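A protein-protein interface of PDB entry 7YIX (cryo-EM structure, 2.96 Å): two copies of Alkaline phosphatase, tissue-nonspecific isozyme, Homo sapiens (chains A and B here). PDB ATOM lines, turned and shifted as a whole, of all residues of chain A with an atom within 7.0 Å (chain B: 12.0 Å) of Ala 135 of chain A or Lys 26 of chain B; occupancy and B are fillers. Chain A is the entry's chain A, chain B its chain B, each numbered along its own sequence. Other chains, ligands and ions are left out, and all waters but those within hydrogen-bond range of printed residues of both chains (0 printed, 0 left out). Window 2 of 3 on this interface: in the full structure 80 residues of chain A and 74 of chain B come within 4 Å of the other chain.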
ATOM      1  N   THR A 105     -31.140 -30.574 -22.718  1.00  0.00           N
ATOM      2  CA  THR A 105     -30.001 -30.419 -21.820  1.00  0.00           C
ATOM      3  C   THR A 105     -29.527 -31.769 -21.297  1.00  0.00           C
ATOM      4  O   THR A 105     -28.320 -32.019 -21.204  1.00  0.00           O
ATOM      5  CB  THR A 105     -30.369 -29.490 -20.664  1.00  0.00           C
ATOM      6  OG1 THR A 105     -30.459 -28.144 -21.144  1.00  0.00           O
ATOM      7  CG2 THR A 105     -29.326 -29.553 -19.564  1.00  0.00           C
ATOM      8  N   LYS A 124     -34.335 -23.925 -22.334  1.00  0.00           N
ATOM      9  CA  LYS A 124     -34.181 -25.369 -22.445  1.00  0.00           C
ATOM     10  C   LYS A 124     -34.108 -26.007 -21.064  1.00  0.00           C
ATOM     11  O   LYS A 124     -33.613 -25.411 -20.104  1.00  0.00           O
ATOM     12  CB  LYS A 124     -32.931 -25.715 -23.251  1.00  0.00           C
ATOM     13  CG  LYS A 124     -33.106 -25.556 -24.750  1.00  0.00           C
ATOM     14  CD  LYS A 124     -31.925 -26.130 -25.508  1.00  0.00           C
ATOM     15  CE  LYS A 124     -32.174 -26.105 -27.002  1.00  0.00           C
ATOM     16  NZ  LYS A 124     -33.273 -27.023 -27.390  1.00  0.00           N
ATOM     17  N   ALA A 125     -34.609 -27.237 -20.966  1.00  0.00           N
ATOM     18  CA  ALA A 125     -34.731 -27.914 -19.686  1.00  0.00           C
ATOM     19  C   ALA A 125     -34.481 -29.402 -19.872  1.00  0.00           C
ATOM     20  O   ALA A 125     -34.279 -29.888 -20.987  1.00  0.00           O
ATOM     21  CB  ALA A 125     -36.108 -27.669 -19.061  1.00  0.00           C
ATOM     22  N   ASN A 126     -34.504 -30.129 -18.758  1.00  0.00           N
ATOM     23  CA  ASN A 126     -34.304 -31.568 -18.774  1.00  0.00           C
ATOM     24  C   ASN A 126     -35.501 -32.255 -19.426  1.00  0.00           C
ATOM     25  O   ASN A 126     -36.458 -31.619 -19.872  1.00  0.00           O
ATOM     26  CB  ASN A 126     -34.093 -32.090 -17.356  1.00  0.00           C
ATOM     27  CG  ASN A 126     -32.722 -31.762 -16.812  1.00  0.00           C
ATOM     28  OD1 ASN A 126     -31.870 -31.232 -17.521  1.00  0.00           O
ATOM     29  ND2 ASN A 126     -32.501 -32.074 -15.541  1.00  0.00           N
ATOM     30  N   VAL A 132     -40.213 -25.934 -15.893  1.00  0.00           N
ATOM     31  CA  VAL A 132     -39.151 -25.634 -14.944  1.00  0.00           C
ATOM     32  C   VAL A 132     -37.817 -25.645 -15.676  1.00  0.00           C
ATOM     33  O   VAL A 132     -37.701 -26.138 -16.799  1.00  0.00           O
ATOM     34  CB  VAL A 132     -39.130 -26.623 -13.763  1.00  0.00           C
ATOM     35  CG1 VAL A 132     -40.300 -26.362 -12.842  1.00  0.00           C
ATOM     36  CG2 VAL A 132     -39.193 -28.037 -14.276  1.00  0.00           C
ATOM     37  N   SER A 133     -36.802 -25.084 -15.024  1.00  0.00           N
ATOM     38  CA  SER A 133     -35.486 -24.942 -15.632  1.00  0.00           C
ATOM     39  C   SER A 133     -34.721 -26.262 -15.531  1.00  0.00           C
ATOM     40  O   SER A 133     -35.259 -27.293 -15.119  1.00  0.00           O
ATOM     41  CB  SER A 133     -34.721 -23.795 -14.981  1.00  0.00           C
ATOM     42  OG  SER A 133     -34.392 -24.100 -13.639  1.00  0.00           O
ATOM     43  N   ALA A 134     -33.447 -26.241 -15.911  1.00  0.00           N
ATOM     44  CA  ALA A 134     -32.618 -27.437 -15.933  1.00  0.00           C
ATOM     45  C   ALA A 134     -31.977 -27.746 -14.589  1.00  0.00           C
ATOM     46  O   ALA A 134     -31.272 -28.753 -14.474  1.00  0.00           O
ATOM     47  CB  ALA A 134     -31.528 -27.302 -17.000  1.00  0.00           C
ATOM     48  N   ALA A 135     -32.196 -26.913 -13.575  1.00  0.00           N
ATOM     49  CA  ALA A 135     -31.613 -27.137 -12.260  1.00  0.00           C
ATOM     50  C   ALA A 135     -32.419 -28.109 -11.411  1.00  0.00           C
ATOM     51  O   ALA A 135     -31.990 -28.436 -10.301  1.00  0.00           O
ATOM     52  CB  ALA A 135     -31.465 -25.808 -11.519  1.00  0.00           C
ATOM     53  N   THR A 136     -33.563 -28.573 -11.900  1.00  0.00           N
ATOM     54  CA  THR A 136     -34.419 -29.498 -11.176  1.00  0.00           C
ATOM     55  C   THR A 136     -34.156 -30.933 -11.619  1.00  0.00           C
ATOM     56  O   THR A 136     -33.643 -31.191 -12.710  1.00  0.00           O
ATOM     57  CB  THR A 136     -35.893 -29.149 -11.392  1.00  0.00           C
ATOM     58  OG1 THR A 136     -36.706 -29.942 -10.521  1.00  0.00           O
ATOM     59  CG2 THR A 136     -36.289 -29.428 -12.822  1.00  0.00           C
ATOM     60  N   GLU A 137     -34.513 -31.869 -10.748  1.00  0.00           N
ATOM     61  CA  GLU A 137     -34.353 -33.290 -11.012  1.00  0.00           C
ATOM     62  C   GLU A 137     -35.723 -33.941 -11.130  1.00  0.00           C
ATOM     63  O   GLU A 137     -36.657 -33.574 -10.411  1.00  0.00           O
ATOM     64  CB  GLU A 137     -33.534 -33.965  -9.910  1.00  0.00           C
ATOM     65  CG  GLU A 137     -32.177 -33.324  -9.686  1.00  0.00           C
ATOM     66  CD  GLU A 137     -31.363 -34.026  -8.618  1.00  0.00           C
ATOM     67  OE1 GLU A 137     -31.824 -35.065  -8.103  1.00  0.00           O
ATOM     68  OE2 GLU A 137     -30.261 -33.538  -8.291  1.00  0.00           O
ATOM     69  N   THR A 143     -37.220 -29.831  -5.157  1.00  0.00           N
ATOM     70  CA  THR A 143     -36.214 -29.176  -5.975  1.00  0.00           C
ATOM     71  C   THR A 143     -36.807 -28.318  -7.085  1.00  0.00           C
ATOM     72  O   THR A 143     -36.049 -27.793  -7.906  1.00  0.00           O
ATOM     73  CB  THR A 143     -35.262 -30.214  -6.589  1.00  0.00           C
ATOM     74  OG1 THR A 143     -34.169 -29.545  -7.229  1.00  0.00           O
ATOM     75  CG2 THR A 143     -35.990 -31.069  -7.604  1.00  0.00           C
ATOM     76  N   THR A 144     -38.129 -28.159  -7.135  1.00  0.00           N
ATOM     77  CA  THR A 144     -38.780 -27.322  -8.133  1.00  0.00           C
ATOM     78  C   THR A 144     -39.150 -25.944  -7.609  1.00  0.00           C
ATOM     79  O   THR A 144     -39.748 -25.157  -8.349  1.00  0.00           O
ATOM     80  CB  THR A 144     -40.040 -28.009  -8.669  1.00  0.00           C
ATOM     81  OG1 THR A 144     -40.594 -27.225  -9.731  1.00  0.00           O
ATOM     82  CG2 THR A 144     -41.077 -28.142  -7.572  1.00  0.00           C
ATOM     83  N   ASN A 147     -37.396 -22.523  -9.291  1.00  0.00           N
ATOM     84  CA  ASN A 147     -36.862 -22.831 -10.612  1.00  0.00           C
ATOM     85  C   ASN A 147     -37.928 -22.761 -11.700  1.00  0.00           C
ATOM     86  O   ASN A 147     -37.708 -23.258 -12.809  1.00  0.00           O
ATOM     87  CB  ASN A 147     -36.202 -24.209 -10.611  1.00  0.00           C
ATOM     88  CG  ASN A 147     -35.066 -24.311  -9.616  1.00  0.00           C
ATOM     89  OD1 ASN A 147     -34.249 -23.400  -9.496  1.00  0.00           O
ATOM     90  ND2 ASN A 147     -35.005 -25.425  -8.900  1.00  0.00           N
ATOM     91  N   LEU B  20     -22.815 -34.096 -20.003  1.00  0.00           N
ATOM     92  CA  LEU B  20     -24.071 -34.402 -19.328  1.00  0.00           C
ATOM     93  C   LEU B  20     -24.498 -33.261 -18.409  1.00  0.00           C
ATOM     94  O   LEU B  20     -24.101 -33.213 -17.244  1.00  0.00           O
ATOM     95  CB  LEU B  20     -23.949 -35.700 -18.528  1.00  0.00           C
ATOM     96  CG  LEU B  20     -25.258 -36.406 -18.164  1.00  0.00           C
ATOM     97  CD1 LEU B  20     -26.189 -36.482 -19.362  1.00  0.00           C
ATOM     98  CD2 LEU B  20     -24.984 -37.792 -17.605  1.00  0.00           C
ATOM     99  N   VAL B  21     -25.312 -32.358 -18.948  1.00  0.00           N
ATOM    100  CA  VAL B  21     -25.848 -31.208 -18.219  1.00  0.00           C
ATOM    101  C   VAL B  21     -24.678 -30.378 -17.697  1.00  0.00           C
ATOM    102  O   VAL B  21     -24.341 -30.458 -16.506  1.00  0.00           O
ATOM    103  CB  VAL B  21     -26.798 -31.650 -17.092  1.00  0.00           C
ATOM    104  CG1 VAL B  21     -27.285 -30.451 -16.276  1.00  0.00           C
ATOM    105  CG2 VAL B  21     -27.971 -32.429 -17.660  1.00  0.00           C
ATOM    106  N   PRO B  22     -23.981 -29.635 -18.557  1.00  0.00           N
ATOM    107  CA  PRO B  22     -22.915 -28.756 -18.066  1.00  0.00           C
ATOM    108  C   PRO B  22     -23.470 -27.713 -17.107  1.00  0.00           C
ATOM    109  O   PRO B  22     -24.630 -27.308 -17.200  1.00  0.00           O
ATOM    110  CB  PRO B  22     -22.368 -28.106 -19.345  1.00  0.00           C
ATOM    111  CG  PRO B  22     -22.834 -28.984 -20.460  1.00  0.00           C
ATOM    112  CD  PRO B  22     -24.146 -29.540 -20.016  1.00  0.00           C
ATOM    113  N   GLU B  23     -22.621 -27.289 -16.169  1.00  0.00           N
ATOM    114  CA  GLU B  23     -23.069 -26.387 -15.112  1.00  0.00           C
ATOM    115  C   GLU B  23     -23.608 -25.081 -15.684  1.00  0.00           C
ATOM    116  O   GLU B  23     -24.670 -24.603 -15.268  1.00  0.00           O
ATOM    117  CB  GLU B  23     -21.916 -26.115 -14.145  1.00  0.00           C
ATOM    118  CG  GLU B  23     -22.271 -25.219 -12.971  1.00  0.00           C
ATOM    119  CD  GLU B  23     -23.285 -25.849 -12.040  1.00  0.00           C
ATOM    120  OE1 GLU B  23     -23.357 -27.094 -11.990  1.00  0.00           O
ATOM    121  OE2 GLU B  23     -24.011 -25.098 -11.353  1.00  0.00           O
ATOM    122  N   LYS B  24     -22.906 -24.508 -16.665  1.00  0.00           N
ATOM    123  CA  LYS B  24     -23.286 -23.213 -17.216  1.00  0.00           C
ATOM    124  C   LYS B  24     -24.684 -23.216 -17.816  1.00  0.00           C
ATOM    125  O   LYS B  24     -25.291 -22.148 -17.948  1.00  0.00           O
ATOM    126  CB  LYS B  24     -22.272 -22.785 -18.279  1.00  0.00           C
ATOM    127  CG  LYS B  24     -22.117 -23.784 -19.413  1.00  0.00           C
ATOM    128  CD  LYS B  24     -20.984 -23.403 -20.348  1.00  0.00           C
ATOM    129  CE  LYS B  24     -21.401 -22.290 -21.290  1.00  0.00           C
ATOM    130  NZ  LYS B  24     -20.355 -22.006 -22.312  1.00  0.00           N
ATOM    131  N   GLU B  25     -25.209 -24.382 -18.178  1.00  0.00           N
ATOM    132  CA  GLU B  25     -26.521 -24.483 -18.799  1.00  0.00           C
ATOM    133  C   GLU B  25     -27.645 -24.664 -17.789  1.00  0.00           C
ATOM    134  O   GLU B  25     -28.799 -24.832 -18.196  1.00  0.00           O
ATOM    135  CB  GLU B  25     -26.539 -25.639 -19.801  1.00  0.00           C
ATOM    136  CG  GLU B  25     -25.630 -25.423 -20.997  1.00  0.00           C
ATOM    137  CD  GLU B  25     -25.695 -26.560 -21.994  1.00  0.00           C
ATOM    138  OE1 GLU B  25     -26.304 -27.600 -21.671  1.00  0.00           O
ATOM    139  OE2 GLU B  25     -25.138 -26.413 -23.102  1.00  0.00           O
ATOM    140  N   LYS B  26     -27.347 -24.631 -16.493  1.00  0.00           N
ATOM    141  CA  LYS B  26     -28.368 -24.812 -15.470  1.00  0.00           C
ATOM    142  C   LYS B  26     -29.075 -23.516 -15.092  1.00  0.00           C
ATOM    143  O   LYS B  26     -29.948 -23.539 -14.220  1.00  0.00           O
ATOM    144  CB  LYS B  26     -27.752 -25.438 -14.217  1.00  0.00           C
ATOM    145  CG  LYS B  26     -27.655 -26.950 -14.264  1.00  0.00           C
ATOM    146  CD  LYS B  26     -26.825 -27.477 -13.110  1.00  0.00           C
ATOM    147  CE  LYS B  26     -26.954 -28.982 -12.974  1.00  0.00           C
ATOM    148  NZ  LYS B  26     -26.183 -29.497 -11.811  1.00  0.00           N
ATOM    149  N   ASP B  27     -28.725 -22.395 -15.718  1.00  0.00           N
ATOM    150  CA  ASP B  27     -29.280 -21.100 -15.365  1.00  0.00           C
ATOM    151  C   ASP B  27     -30.062 -20.532 -16.543  1.00  0.00           C
ATOM    152  O   ASP B  27     -29.528 -20.468 -17.658  1.00  0.00           O
ATOM    153  CB  ASP B  27     -28.161 -20.129 -14.955  1.00  0.00           C
ATOM    154  CG  ASP B  27     -28.667 -18.978 -14.111  1.00  0.00           C
ATOM    155  OD1 ASP B  27     -29.020 -19.211 -12.937  1.00  0.00           O
ATOM    156  OD2 ASP B  27     -28.707 -17.838 -14.617  1.00  0.00           O
ATOM    157  N   PRO B  28     -31.319 -20.122 -16.346  1.00  0.00           N
ATOM    158  CA  PRO B  28     -32.116 -19.625 -17.480  1.00  0.00           C
ATOM    159  C   PRO B  28     -31.541 -18.386 -18.144  1.00  0.00           C
ATOM    160  O   PRO B  28     -31.790 -18.159 -19.338  1.00  0.00           O
ATOM    161  CB  PRO B  28     -33.483 -19.334 -16.844  1.00  0.00           C
ATOM    162  CG  PRO B  28     -33.491 -20.090 -15.556  1.00  0.00           C
ATOM    163  CD  PRO B  28     -32.076 -20.102 -15.087  1.00  0.00           C
ATOM    164  N   LYS B  29     -30.789 -17.570 -17.401  1.00  0.00           N
ATOM    165  CA  LYS B  29     -30.221 -16.355 -17.973  1.00  0.00           C
ATOM    166  C   LYS B  29     -29.310 -16.664 -19.150  1.00  0.00           C
ATOM    167  O   LYS B  29     -29.238 -15.879 -20.099  1.00  0.00           O
ATOM    168  CB  LYS B  29     -29.458 -15.580 -16.900  1.00  0.00           C
ATOM    169  CG  LYS B  29     -29.020 -14.194 -17.330  1.00  0.00           C
ATOM    170  CD  LYS B  29     -28.267 -13.483 -16.220  1.00  0.00           C
ATOM    171  CE  LYS B  29     -27.912 -12.062 -16.622  1.00  0.00           C
ATOM    172  NZ  LYS B  29     -26.949 -12.031 -17.758  1.00  0.00           N
ATOM    173  N   TYR B  30     -28.621 -17.806 -19.114  1.00  0.00           N
ATOM    174  CA  TYR B  30     -27.761 -18.207 -20.224  1.00  0.00           C
ATOM    175  C   TYR B  30     -28.559 -18.343 -21.516  1.00  0.00           C
ATOM    176  O   TYR B  30     -28.212 -17.747 -22.546  1.00  0.00           O
ATOM    177  CB  TYR B  30     -27.065 -19.520 -19.860  1.00  0.00           C
ATOM    178  CG  TYR B  30     -26.258 -20.164 -20.960  1.00  0.00           C
ATOM    179  CD1 TYR B  30     -24.981 -19.720 -21.261  1.00  0.00           C
ATOM    180  CD2 TYR B  30     -26.761 -21.239 -21.675  1.00  0.00           C
ATOM    181  CE1 TYR B  30     -24.237 -20.316 -22.258  1.00  0.00           C
ATOM    182  CE2 TYR B  30     -26.026 -21.839 -22.671  1.00  0.00           C
ATOM    183  CZ  TYR B  30     -24.767 -21.375 -22.959  1.00  0.00           C
ATOM    184  OH  TYR B  30     -24.032 -21.976 -23.953  1.00  0.00           O
ATOM    185  N   TRP B  31     -29.654 -19.105 -21.470  1.00  0.00           N
ATOM    186  CA  TRP B  31     -30.474 -19.309 -22.660  1.00  0.00           C
ATOM    187  C   TRP B  31     -31.150 -18.018 -23.098  1.00  0.00           C
ATOM    188  O   TRP B  31     -31.260 -17.746 -24.300  1.00  0.00           O
ATOM    189  CB  TRP B  31     -31.510 -20.397 -22.394  1.00  0.00           C
ATOM    190  CG  TRP B  31     -30.910 -21.678 -21.919  1.00  0.00           C
ATOM    191  CD1 TRP B  31     -30.905 -22.156 -20.644  1.00  0.00           C
ATOM    192  CD2 TRP B  31     -30.222 -22.647 -22.714  1.00  0.00           C
ATOM    193  NE1 TRP B  31     -30.256 -23.365 -20.595  1.00  0.00           N
ATOM    194  CE2 TRP B  31     -29.827 -23.687 -21.855  1.00  0.00           C
ATOM    195  CE3 TRP B  31     -29.902 -22.736 -24.072  1.00  0.00           C
ATOM    196  CZ2 TRP B  31     -29.131 -24.804 -22.307  1.00  0.00           C
ATOM    197  CZ3 TRP B  31     -29.211 -23.842 -24.518  1.00  0.00           C
ATOM    198  CH2 TRP B  31     -28.833 -24.861 -23.640  1.00  0.00           C
ATOM    199  N   ARG B  32     -31.618 -17.213 -22.141  1.00  0.00           N
ATOM    200  CA  ARG B  32     -32.258 -15.952 -22.503  1.00  0.00           C
ATOM    201  C   ARG B  32     -31.279 -15.012 -23.201  1.00  0.00           C
ATOM    202  O   ARG B  32     -31.623 -14.386 -24.210  1.00  0.00           O
ATOM    203  CB  ARG B  32     -32.861 -15.295 -21.264  1.00  0.00           C
ATOM    204  CG  ARG B  32     -33.968 -16.117 -20.627  1.00  0.00           C
ATOM    205  CD  ARG B  32     -34.527 -15.453 -19.383  1.00  0.00           C
ATOM    206  NE  ARG B  32     -35.841 -15.981 -19.036  1.00  0.00           N
ATOM    207  CZ  ARG B  32     -36.174 -16.439 -17.838  1.00  0.00           C
ATOM    208  NH1 ARG B  32     -35.310 -16.447 -16.836  1.00  0.00           N
ATOM    209  NH2 ARG B  32     -37.405 -16.899 -17.637  1.00  0.00           N
ATOM    210  N   ASP B  33     -30.050 -14.912 -22.688  1.00  0.00           N
ATOM    211  CA  ASP B  33     -29.042 -14.068 -23.324  1.00  0.00           C
ATOM    212  C   ASP B  33     -28.679 -14.587 -24.708  1.00  0.00           C
ATOM    213  O   ASP B  33     -28.495 -13.800 -25.645  1.00  0.00           O
ATOM    214  CB  ASP B  33     -27.798 -13.985 -22.442  1.00  0.00           C
ATOM    215  CG  ASP B  33     -28.048 -13.238 -21.153  1.00  0.00           C
ATOM    216  OD1 ASP B  33     -29.176 -12.736 -20.967  1.00  0.00           O
ATOM    217  OD2 ASP B  33     -27.118 -13.150 -20.324  1.00  0.00           O
ATOM    218  N   GLN B  34     -28.560 -15.909 -24.854  1.00  0.00           N
ATOM    219  CA  GLN B  34     -28.288 -16.484 -26.168  1.00  0.00           C
ATOM    220  C   GLN B  34     -29.379 -16.110 -27.165  1.00  0.00           C
ATOM    221  O   GLN B  34     -29.094 -15.684 -28.294  1.00  0.00           O
ATOM    222  CB  GLN B  34     -28.166 -18.003 -26.045  1.00  0.00           C
ATOM    223  CG  GLN B  34     -27.241 -18.649 -27.052  1.00  0.00           C
ATOM    224  CD  GLN B  34     -27.125 -20.144 -26.844  1.00  0.00           C
ATOM    225  OE1 GLN B  34     -28.125 -20.834 -26.651  1.00  0.00           O
ATOM    226  NE2 GLN B  34     -25.901 -20.653 -26.881  1.00  0.00           N
ATOM    227  N   GLU B  86     -24.332 -28.913 -29.601  1.00  0.00           N
ATOM    228  CA  GLU B  86     -24.393 -27.463 -29.714  1.00  0.00           C
ATOM    229  C   GLU B  86     -23.423 -26.889 -30.738  1.00  0.00           C
ATOM    230  O   GLU B  86     -23.517 -25.698 -31.051  1.00  0.00           O
ATOM    231  CB  GLU B  86     -24.113 -26.824 -28.353  1.00  0.00           C
ATOM    232  CG  GLU B  86     -22.674 -26.970 -27.905  1.00  0.00           C
ATOM    233  CD  GLU B  86     -22.469 -28.165 -27.002  1.00  0.00           C
ATOM    234  OE1 GLU B  86     -23.270 -29.118 -27.087  1.00  0.00           O
ATOM    235  OE2 GLU B  86     -21.501 -28.156 -26.213  1.00  0.00           O
ATOM    236  N   ARG B 393     -27.063 -37.447 -23.421  1.00  0.00           N
ATOM    237  CA  ARG B 393     -26.182 -36.391 -23.896  1.00  0.00           C
ATOM    238  C   ARG B 393     -24.728 -36.840 -23.843  1.00  0.00           C
ATOM    239  O   ARG B 393     -24.288 -37.465 -22.875  1.00  0.00           O
ATOM    240  CB  ARG B 393     -26.366 -35.127 -23.060  1.00  0.00           C
ATOM    241  CG  ARG B 393     -25.672 -33.905 -23.626  1.00  0.00           C
ATOM    242  CD  ARG B 393     -26.638 -33.034 -24.402  1.00  0.00           C
ATOM    243  NE  ARG B 393     -25.997 -31.829 -24.912  1.00  0.00           N
ATOM    244  CZ  ARG B 393     -25.754 -30.746 -24.187  1.00  0.00           C
ATOM    245  NH1 ARG B 393     -26.089 -30.680 -22.909  1.00  0.00           N
ATOM    246  NH2 ARG B 393     -25.159 -29.703 -24.758  1.00  0.00           N
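O of Thr 105 of chain A sits at hydrogen-bond distance from NH1 of Arg 393 of chain B, 3.1 Å away.
The backbone NH (N) of Ser 133 of chain A lies within hydrogen-bond range of the backbone carbonyl oxygen (O) of Asn 147 of chain A.
NZ of Lys 26 of chain B lies within salt-bridge range of OE1 of Glu 23 of chain B (3.7 Å).
The indole nitrogen (NE1) of Trp 31 of chain B is in hydrogen-bond range of the backbone carbonyl oxygen (O) of Glu 25 of chain B (3.2 Å).
The guanidinium group (NH1) of Arg 393 of chain B is in salt-bridge range of the side-chain carboxylate (OE1) of Glu 25 of chain B (3.3 Å).
The guanidinium group (NH2) of Arg 393 of chain B lies within salt-bridge range of the side-chain carboxylate (OE1) of Glu 86 of chain B, 3.1 Å away.
O of Thr 105 of chain A touches CG2 of Val 21 of chain B, at 3.6 Å.
Trp 31 of chain B touches Thr 105 of chain A (CZ2 to OG1, 3.8 Å).
CD of Lys 124 of chain A touches CZ3 of Trp 31 of chain B, at 3.7 Å.
Ser 133 of chain A touches Pro 28 of chain B (CB to CG, 3.9 Å).
Ala 134 of chain A touches Glu 25 of chain B.
Lys 26 of chain B touches Ala 135 of chain A (O to CB, 3.8 Å).
Ala 135 of chain A touches just one residue of chain B: Lys 26 (3.8 Å).
Of chain A, only Ala 135 comes within 4 Å of Lys 26 of chain B.
Of chain B, only Pro 28 comes within 4 Å of Ser 133 of chain A.
No residue of chain B comes within 4 Å of Glu 137 of chain A.
No residue of chain B comes within 4 Å of Thr 143 of chain A.
Asn 147 of chain A touches none of the printed residues of chain B.
Printed residues of chain A within 4 Å of Glu 25 of chain B: Ala 134.
Printed residues of chain A within 4 Å of Pro 28 of chain B: Ser 133.
Printed residues of chain B within 4 Å of Lys 124 of chain A: Trp 31 (3.7 Å).
Printed residues of chain A within 4 Å of Arg 393 of chain B: Thr 105 (3.1 Å).
The nearest residue of chain B that does not touch Ala 135 of chain A is Asp 27 of chain B (6.1 Å).
The nearest printed residue of chain A that does not touch Glu 25 of chain B is Thr 105 of chain A (4.2 Å).
Of the 17 printed residues of chain B, 6 touch a printed residue of chain A.
Hydrophobic or aromatic side chains of chain B that line the printed part of chain A: Val 21, Pro 28 and Trp 31.
Of the 13 printed residues of chain A, 5 touch a printed residue of chain B.
Printed residues of chain A that touch a printed residue of chain B: Thr 105, Lys 124, Ser 133, Ala 134 and Ala 135.
Along chain A the printed residues that touch a printed residue of chain B span positions 105 to 135.
No position is printed for both chains.
Of the 7 pairs that touch across the chains among the printed residues, none has its exchanged pair printed and touching as well.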
